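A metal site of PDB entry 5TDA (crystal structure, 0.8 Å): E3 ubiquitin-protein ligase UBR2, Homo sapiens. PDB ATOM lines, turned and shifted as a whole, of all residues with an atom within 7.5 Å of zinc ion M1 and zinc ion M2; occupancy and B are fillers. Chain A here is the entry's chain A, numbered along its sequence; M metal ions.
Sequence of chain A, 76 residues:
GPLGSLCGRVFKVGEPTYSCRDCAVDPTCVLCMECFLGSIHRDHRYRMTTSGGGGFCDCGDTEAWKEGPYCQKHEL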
ATOM      1  N   SER A   5     -28.676  -6.543  -3.835  1.00  0.00           N
ATOM      2  CA  SER A   5     -29.887  -7.123  -4.391  1.00  0.00           C
ATOM      3  C   SER A   5     -29.571  -8.269  -5.338  1.00  0.00           C
ATOM      4  O   SER A   5     -30.413  -9.126  -5.575  1.00  0.00           O
ATOM      5  CB  SER A   5     -30.720  -6.040  -5.090  1.00  0.00           C
ATOM      6  N   LEU A   6     -28.350  -8.282  -5.878  1.00  0.00           N
ATOM      7  CA  LEU A   6     -27.842  -9.373  -6.704  1.00  0.00           C
ATOM      8  C   LEU A   6     -26.801 -10.161  -5.908  1.00  0.00           C
ATOM      9  O   LEU A   6     -26.437  -9.781  -4.787  1.00  0.00           O
ATOM     10  CB  LEU A   6     -27.243  -8.840  -8.007  1.00  0.00           C
ATOM     11  CG  LEU A   6     -28.219  -8.164  -8.984  1.00  0.00           C
ATOM     12  CD1 LEU A   6     -27.482  -7.754 -10.248  1.00  0.00           C
ATOM     13  CD2 LEU A   6     -29.384  -9.074  -9.333  1.00  0.00           C
ATOM     14  N   CYS A   7     -26.340 -11.273  -6.480  1.00  0.00           N
ATOM     15  CA  CYS A   7     -25.471 -12.183  -5.742  1.00  0.00           C
ATOM     16  C   CYS A   7     -24.031 -11.656  -5.659  1.00  0.00           C
ATOM     17  O   CYS A   7     -23.594 -11.174  -4.609  1.00  0.00           O
ATOM     18  CB  CYS A   7     -25.503 -13.592  -6.363  1.00  0.00           C
ATOM     19  SG  CYS A   7     -24.475 -14.743  -5.393  1.00  0.00           S
ATOM     20  N   GLY A   8     -23.291 -11.769  -6.750  1.00  0.00           N
ATOM     21  CA  GLY A   8     -21.904 -11.320  -6.770  1.00  0.00           C
ATOM     22  C   GLY A   8     -20.924 -12.119  -5.926  1.00  0.00           C
ATOM     23  O   GLY A   8     -19.808 -11.653  -5.679  1.00  0.00           O
ATOM     24  N   ARG A   9     -21.300 -13.317  -5.473  1.00  0.00           N
ATOM     25  CA  ARG A   9     -20.415 -14.114  -4.631  1.00  0.00           C
ATOM     26  C   ARG A   9     -19.144 -14.466  -5.389  1.00  0.00           C
ATOM     27  O   ARG A   9     -19.171 -14.888  -6.545  1.00  0.00           O
ATOM     28  CB  ARG A   9     -21.141 -15.382  -4.126  1.00  0.00           C
ATOM     29  CG  ARG A   9     -22.046 -15.105  -2.884  1.00  0.00           C
ATOM     30  CD  ARG A   9     -22.997 -16.242  -2.469  1.00  0.00           C
ATOM     31  NE  ARG A   9     -22.298 -17.498  -2.184  1.00  0.00           N
ATOM     32  CZ  ARG A   9     -22.830 -18.546  -1.575  1.00  0.00           C
ATOM     33  NH1 ARG A   9     -22.110 -19.627  -1.421  1.00  0.00           N
ATOM     34  NH2 ARG A   9     -24.077 -18.523  -1.111  1.00  0.00           N
ATOM     35  N   PHE A  11     -16.269 -17.212  -5.210  1.00  0.00           N
ATOM     36  CA  PHE A  11     -16.202 -18.533  -4.610  1.00  0.00           C
ATOM     37  C   PHE A  11     -15.019 -18.656  -3.657  1.00  0.00           C
ATOM     38  O   PHE A  11     -13.902 -18.184  -3.940  1.00  0.00           O
ATOM     39  CB  PHE A  11     -16.079 -19.618  -5.684  1.00  0.00           C
ATOM     40  CG  PHE A  11     -17.242 -19.649  -6.644  1.00  0.00           C
ATOM     41  CD1 PHE A  11     -18.545 -19.846  -6.215  1.00  0.00           C
ATOM     42  CD2 PHE A  11     -17.021 -19.483  -7.991  1.00  0.00           C
ATOM     43  CE1 PHE A  11     -19.593 -19.860  -7.131  1.00  0.00           C
ATOM     44  CE2 PHE A  11     -18.058 -19.506  -8.910  1.00  0.00           C
ATOM     45  CZ  PHE A  11     -19.336 -19.692  -8.488  1.00  0.00           C
ATOM     46  N   GLU A  15     -15.919 -24.493  -1.894  1.00  0.00           N
ATOM     47  CA  GLU A  15     -17.326 -24.165  -2.031  1.00  0.00           C
ATOM     48  C   GLU A  15     -17.945 -24.940  -3.192  1.00  0.00           C
ATOM     49  O   GLU A  15     -17.380 -24.952  -4.286  1.00  0.00           O
ATOM     50  CB  GLU A  15     -17.424 -22.672  -2.301  1.00  0.00           C
ATOM     51  CG  GLU A  15     -18.839 -22.199  -2.345  1.00  0.00           C
ATOM     52  CD  GLU A  15     -18.975 -20.707  -2.411  1.00  0.00           C
ATOM     53  OE1 GLU A  15     -20.079 -20.294  -2.833  1.00  0.00           O
ATOM     54  OE2 GLU A  15     -18.057 -19.949  -2.038  1.00  0.00           O
ATOM     55  N   VAL A  30     -21.498 -20.376 -14.250  1.00  0.00           N
ATOM     56  CA  VAL A  30     -21.661 -21.154 -13.027  1.00  0.00           C
ATOM     57  C   VAL A  30     -22.487 -20.360 -12.013  1.00  0.00           C
ATOM     58  O   VAL A  30     -22.617 -19.134 -12.099  1.00  0.00           O
ATOM     59  CB  VAL A  30     -20.297 -21.538 -12.386  1.00  0.00           C
ATOM     60  CG1 VAL A  30     -19.667 -22.700 -13.130  1.00  0.00           C
ATOM     61  CG2 VAL A  30     -19.364 -20.325 -12.304  1.00  0.00           C
ATOM     62  N   LEU A  31     -23.027 -21.098 -11.044  1.00  0.00           N
ATOM     63  CA  LEU A  31     -23.828 -20.566  -9.947  1.00  0.00           C
ATOM     64  C   LEU A  31     -23.297 -21.117  -8.610  1.00  0.00           C
ATOM     65  O   LEU A  31     -22.853 -22.259  -8.522  1.00  0.00           O
ATOM     66  CB  LEU A  31     -25.301 -21.001 -10.075  1.00  0.00           C
ATOM     67  CG  LEU A  31     -26.018 -20.499 -11.329  1.00  0.00           C
ATOM     68  CD1 LEU A  31     -27.375 -21.161 -11.502  1.00  0.00           C
ATOM     69  CD2 LEU A  31     -26.166 -18.983 -11.318  1.00  0.00           C
ATOM     70  N   CYS A  32     -23.378 -20.275  -7.590  1.00  0.00           N
ATOM     71  CA  CYS A  32     -23.195 -20.738  -6.225  1.00  0.00           C
ATOM     72  C   CYS A  32     -24.359 -21.653  -5.834  1.00  0.00           C
ATOM     73  O   CYS A  32     -25.380 -21.729  -6.513  1.00  0.00           O
ATOM     74  CB  CYS A  32     -23.041 -19.556  -5.258  1.00  0.00           C
ATOM     75  SG  CYS A  32     -24.596 -18.650  -4.904  1.00  0.00           S
ATOM     76  N   MET A  33     -24.212 -22.341  -4.692  1.00  0.00           N
ATOM     77  CA  MET A  33     -25.227 -23.302  -4.287  1.00  0.00           C
ATOM     78  C   MET A  33     -26.552 -22.621  -3.962  1.00  0.00           C
ATOM     79  O   MET A  33     -27.626 -23.159  -4.273  1.00  0.00           O
ATOM     80  CB  MET A  33     -24.699 -24.075  -3.080  1.00  0.00           C
ATOM     81  CG  MET A  33     -25.434 -25.335  -2.825  1.00  0.00           C
ATOM     82  SD  MET A  33     -24.499 -26.312  -1.657  1.00  0.00           S
ATOM     83  CE  MET A  33     -25.643 -27.682  -1.449  1.00  0.00           C
ATOM     84  N   GLU A  34     -26.494 -21.459  -3.287  1.00  0.00           N
ATOM     85  CA  GLU A  34     -27.703 -20.711  -2.957  1.00  0.00           C
ATOM     86  C   GLU A  34     -28.499 -20.396  -4.226  1.00  0.00           C
ATOM     87  O   GLU A  34     -29.729 -20.585  -4.289  1.00  0.00           O
ATOM     88  CB  GLU A  34     -27.300 -19.407  -2.251  1.00  0.00           C
ATOM     89  CG  GLU A  34     -28.460 -18.452  -1.962  1.00  0.00           C
ATOM     90  CD  GLU A  34     -28.037 -17.137  -1.310  1.00  0.00           C
ATOM     91  OE1 GLU A  34     -26.818 -16.824  -1.281  1.00  0.00           O
ATOM     92  OE2 GLU A  34     -28.929 -16.405  -0.821  1.00  0.00           O
ATOM     93  N   CYS A  35     -27.812 -19.912  -5.250  1.00  0.00           N
ATOM     94  CA  CYS A  35     -28.503 -19.514  -6.474  1.00  0.00           C
ATOM     95  C   CYS A  35     -28.936 -20.721  -7.294  1.00  0.00           C
ATOM     96  O   CYS A  35     -30.050 -20.744  -7.834  1.00  0.00           O
ATOM     97  CB  CYS A  35     -27.610 -18.555  -7.271  1.00  0.00           C
ATOM     98  SG  CYS A  35     -27.319 -17.009  -6.340  1.00  0.00           S
ATOM     99  N   PHE A  36     -28.086 -21.759  -7.374  1.00  0.00           N
ATOM    100  CA  PHE A  36     -28.479 -22.958  -8.121  1.00  0.00           C
ATOM    101  C   PHE A  36     -29.760 -23.566  -7.549  1.00  0.00           C
ATOM    102  O   PHE A  36     -30.727 -23.823  -8.288  1.00  0.00           O
ATOM    103  CB  PHE A  36     -27.339 -23.987  -8.106  1.00  0.00           C
ATOM    104  CG  PHE A  36     -27.709 -25.269  -8.803  1.00  0.00           C
ATOM    105  CD1 PHE A  36     -27.808 -25.307 -10.185  1.00  0.00           C
ATOM    106  CD2 PHE A  36     -28.007 -26.413  -8.081  1.00  0.00           C
ATOM    107  CE1 PHE A  36     -28.173 -26.474 -10.842  1.00  0.00           C
ATOM    108  CE2 PHE A  36     -28.379 -27.594  -8.724  1.00  0.00           C
ATOM    109  CZ  PHE A  36     -28.462 -27.621 -10.116  1.00  0.00           C
ATOM    110  N   GLY A  38     -32.010 -22.301  -5.678  1.00  0.00           N
ATOM    111  CA  GLY A  38     -33.134 -21.382  -5.763  1.00  0.00           C
ATOM    112  C   GLY A  38     -33.556 -21.044  -7.177  1.00  0.00           C
ATOM    113  O   GLY A  38     -34.408 -20.164  -7.356  1.00  0.00           O
ATOM    114  N   SER A  39     -33.008 -21.742  -8.178  1.00  0.00           N
ATOM    115  CA  SER A  39     -33.274 -21.472  -9.581  1.00  0.00           C
ATOM    116  C   SER A  39     -33.999 -22.651 -10.223  1.00  0.00           C
ATOM    117  O   SER A  39     -34.070 -23.763  -9.651  1.00  0.00           O
ATOM    118  CB  SER A  39     -31.955 -21.237 -10.350  1.00  0.00           C
ATOM    119  OG  SER A  39     -31.283 -22.454 -10.622  1.00  0.00           O
ATOM    120  N   PHE A  56     -16.579 -16.380  -9.774  1.00  0.00           N
ATOM    121  CA  PHE A  56     -17.767 -15.742  -9.214  1.00  0.00           C
ATOM    122  C   PHE A  56     -19.057 -16.367  -9.749  1.00  0.00           C
ATOM    123  O   PHE A  56     -19.109 -16.942 -10.844  1.00  0.00           O
ATOM    124  CB  PHE A  56     -17.747 -14.219  -9.440  1.00  0.00           C
ATOM    125  CG  PHE A  56     -17.682 -13.819 -10.905  1.00  0.00           C
ATOM    126  CD1 PHE A  56     -16.458 -13.653 -11.552  1.00  0.00           C
ATOM    127  CD2 PHE A  56     -18.853 -13.575 -11.615  1.00  0.00           C
ATOM    128  CE1 PHE A  56     -16.406 -13.272 -12.894  1.00  0.00           C
ATOM    129  CE2 PHE A  56     -18.800 -13.173 -12.950  1.00  0.00           C
ATOM    130  CZ  PHE A  56     -17.570 -13.015 -13.587  1.00  0.00           C
ATOM    131  N   CYS A  57     -20.112 -16.180  -8.954  1.00  0.00           N
ATOM    132  CA  CYS A  57     -21.443 -16.619  -9.341  1.00  0.00           C
ATOM    133  C   CYS A  57     -22.016 -15.723 -10.451  1.00  0.00           C
ATOM    134  O   CYS A  57     -21.933 -14.490 -10.377  1.00  0.00           O
ATOM    135  CB  CYS A  57     -22.351 -16.548  -8.095  1.00  0.00           C
ATOM    136  SG  CYS A  57     -24.047 -17.083  -8.464  1.00  0.00           S
ATOM    137  N   ASP A  58     -22.619 -16.357 -11.465  1.00  0.00           N
ATOM    138  CA  ASP A  58     -23.192 -15.670 -12.614  1.00  0.00           C
ATOM    139  C   ASP A  58     -24.701 -15.425 -12.497  1.00  0.00           C
ATOM    140  O   ASP A  58     -25.352 -15.090 -13.494  1.00  0.00           O
ATOM    141  CB  ASP A  58     -22.868 -16.439 -13.902  1.00  0.00           C
ATOM    142  CG  ASP A  58     -21.363 -16.534 -14.156  1.00  0.00           C
ATOM    143  OD1 ASP A  58     -20.713 -15.452 -14.123  1.00  0.00           O
ATOM    144  OD2 ASP A  58     -20.856 -17.645 -14.362  1.00  0.00           O
ATOM    145  N   CYS A  59     -25.266 -15.577 -11.295  1.00  0.00           N
ATOM    146  CA  CYS A  59     -26.689 -15.267 -11.115  1.00  0.00           C
ATOM    147  C   CYS A  59     -26.920 -13.803 -11.480  1.00  0.00           C
ATOM    148  O   CYS A  59     -26.206 -12.917 -11.011  1.00  0.00           O
ATOM    149  CB  CYS A  59     -27.081 -15.519  -9.656  1.00  0.00           C
ATOM    150  SG  CYS A  59     -28.825 -15.111  -9.335  1.00  0.00           S
ATOM    151  N   GLY A  60     -27.944 -13.555 -12.306  1.00  0.00           N
ATOM    152  CA  GLY A  60     -28.287 -12.216 -12.716  1.00  0.00           C
ATOM    153  C   GLY A  60     -27.660 -11.745 -14.005  1.00  0.00           C
ATOM    154  O   GLY A  60     -28.088 -10.714 -14.537  1.00  0.00           O
ATOM    155  N   PRO A  69     -32.122 -16.733 -15.800  1.00  0.00           N
ATOM    156  CA  PRO A  69     -30.871 -16.016 -15.479  1.00  0.00           C
ATOM    157  C   PRO A  69     -30.724 -15.613 -14.028  1.00  0.00           C
ATOM    158  O   PRO A  69     -29.621 -15.194 -13.640  1.00  0.00           O
ATOM    159  CB  PRO A  69     -30.924 -14.784 -16.383  1.00  0.00           C
ATOM    160  CG  PRO A  69     -32.377 -14.542 -16.552  1.00  0.00           C
ATOM    161  CD  PRO A  69     -33.018 -15.919 -16.632  1.00  0.00           C
ATOM    162  N   TYR A  70     -31.801 -15.688 -13.232  1.00  0.00           N
ATOM    163  CA  TYR A  70     -31.834 -15.319 -11.832  1.00  0.00           C
ATOM    164  C   TYR A  70     -32.347 -16.499 -11.000  1.00  0.00           C
ATOM    165  O   TYR A  70     -32.972 -17.436 -11.503  1.00  0.00           O
ATOM    166  CB  TYR A  70     -32.777 -14.106 -11.583  1.00  0.00           C
ATOM    167  CG  TYR A  70     -32.317 -12.766 -12.151  1.00  0.00           C
ATOM    168  CD1 TYR A  70     -32.598 -12.422 -13.474  1.00  0.00           C
ATOM    169  CD2 TYR A  70     -31.650 -11.842 -11.371  1.00  0.00           C
ATOM    170  CE1 TYR A  70     -32.196 -11.201 -13.995  1.00  0.00           C
ATOM    171  CE2 TYR A  70     -31.252 -10.620 -11.879  1.00  0.00           C
ATOM    172  CZ  TYR A  70     -31.529 -10.299 -13.192  1.00  0.00           C
ATOM    173  OH  TYR A  70     -31.121  -9.085 -13.702  1.00  0.00           O
ATOM    174  N   CYS A  71     -32.049 -16.466  -9.701  1.00  0.00           N
ATOM    175  CA  CYS A  71     -32.696 -17.329  -8.730  1.00  0.00           C
ATOM    176  C   CYS A  71     -33.790 -16.548  -7.999  1.00  0.00           C
ATOM    177  O   CYS A  71     -33.956 -15.338  -8.178  1.00  0.00           O
ATOM    178  CB  CYS A  71     -31.682 -17.868  -7.734  1.00  0.00           C
ATOM    179  SG  CYS A  71     -31.141 -16.621  -6.523  1.00  0.00           S
ATOM    180  N   GLN A  72     -34.502 -17.273  -7.148  1.00  0.00           N
ATOM    181  CA  GLN A  72     -35.638 -16.693  -6.456  1.00  0.00           C
ATOM    182  C   GLN A  72     -35.216 -15.577  -5.493  1.00  0.00           C
ATOM    183  O   GLN A  72     -36.002 -14.642  -5.273  1.00  0.00           O
ATOM    184  CB  GLN A  72     -36.396 -17.825  -5.760  1.00  0.00           C
ATOM    185  CG  GLN A  72     -37.719 -17.452  -5.215  1.00  0.00           C
ATOM    186  CD  GLN A  72     -37.596 -16.959  -3.807  1.00  0.00           C
ATOM    187  OE1 GLN A  72     -36.568 -17.128  -3.172  1.00  0.00           O
ATOM    188  NE2 GLN A  72     -38.675 -16.382  -3.283  1.00  0.00           N
ATOM    189  N   LYS A  73     -33.995 -15.629  -4.927  1.00  0.00           N
ATOM    190  CA  LYS A  73     -33.513 -14.581  -4.015  1.00  0.00           C
ATOM    191  C   LYS A  73     -33.167 -13.279  -4.738  1.00  0.00           C
ATOM    192  O   LYS A  73     -33.292 -12.195  -4.157  1.00  0.00           O
ATOM    193  CB  LYS A  73     -32.238 -15.050  -3.279  1.00  0.00           C
ATOM    194  CG  LYS A  73     -32.465 -16.033  -2.154  1.00  0.00           C
ATOM    195  CD  LYS A  73     -33.115 -15.390  -0.946  1.00  0.00           C
ATOM    196  CE  LYS A  73     -32.670 -16.083   0.355  1.00  0.00           C
ATOM    197  NZ  LYS A  73     -31.270 -15.735   0.779  1.00  0.00           N
ATOM    198  N   HIS A  74     -32.683 -13.357  -5.968  1.00  0.00           N
ATOM    199  CA  HIS A  74     -32.082 -12.198  -6.628  1.00  0.00           C
ATOM    200  C   HIS A  74     -32.930 -11.630  -7.750  1.00  0.00           C
ATOM    201  O   HIS A  74     -32.563 -10.589  -8.316  1.00  0.00           O
ATOM    202  CB  HIS A  74     -30.654 -12.510  -7.074  1.00  0.00           C
ATOM    203  CG  HIS A  74     -29.773 -12.883  -5.923  1.00  0.00           C
ATOM    204  ND1 HIS A  74     -29.136 -14.100  -5.811  1.00  0.00           N
ATOM    205  CD2 HIS A  74     -29.529 -12.203  -4.777  1.00  0.00           C
ATOM    206  CE1 HIS A  74     -28.504 -14.131  -4.643  1.00  0.00           C
ATOM    207  NE2 HIS A  74     -28.718 -12.996  -3.998  1.00  0.00           N
ATOM    208  N   GLU A  75     -34.096 -12.246  -8.019  1.00  0.00           N
ATOM    209  CA  GLU A  75     -34.983 -11.772  -9.074  1.00  0.00           C
ATOM    210  C   GLU A  75     -35.639 -10.442  -8.699  1.00  0.00           C
ATOM    211  O   GLU A  75     -36.189  -9.757  -9.572  1.00  0.00           O
ATOM    212  CB  GLU A  75     -36.064 -12.810  -9.358  1.00  0.00           C
ATOM    213  CG  GLU A  75     -36.936 -13.177  -8.178  1.00  0.00           C
ATOM    214  CD  GLU A  75     -37.897 -14.293  -8.506  1.00  0.00           C
ATOM    215  OE1 GLU A  75     -38.093 -14.537  -9.707  1.00  0.00           O
ATOM    216  OE2 GLU A  75     -38.436 -14.924  -7.581  1.00  0.00           O
HETATM  217 ZN    ZN M   1     -29.092 -15.682  -7.113  1.00  0.00          ZN
HETATM  218 ZN    ZN M   2     -24.940 -16.819  -6.321  1.00  0.00          ZN
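SG of Cys 7 sits close to N of Arg 9, at 3.5 Å.
The side-chain sulfur (SG) of Cys 57 sits close to the backbone NH (N) of Cys 59 (3.4 Å).
O of Arg 9 sits at hydrogen-bond distance from N of Cys 57.
SG of Cys 32 sits close to N of Glu 34, at 3.8 Å.
The side-chain sulfur (SG) of Cys 32 lies close to the guanidinium group (NE) of Arg 9.
The backbone carbonyl oxygen (O) of Cys 35 sits close to the side-chain hydroxyl (OG) of Ser 39.
The side-chain sulfur (SG) of Cys 71 sits close to the backbone NH (N) of Lys 73.
Zinc ion M1 is bound by ND1 of His 74, 2.0 Å away.
Zinc ion M1 is bound by SG of Cys 59 (2.3 Å).
Zinc ion M1 is bound by SG of Cys 71.
SG of Cys 35 is bound to zinc ion M1 (2.3 Å).
Within 4 Å of zinc ion M2: Cys 7, Cys 32, Cys 35 and Cys 57.
Within 4 Å of zinc ion M1: Cys 35, Cys 59, Cys 71 and His 74.
Zinc ion M2 is bound by the side-chain sulfur of Cys 7 (2.3 Å), the side-chain sulfur of Cys 57 (2.3 Å), the side-chain sulfur of Cys 32 (2.3 Å) and the side-chain sulfur of Cys 35 (2.4 Å).
Zinc ion M2 has four donor atoms within binding distance.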
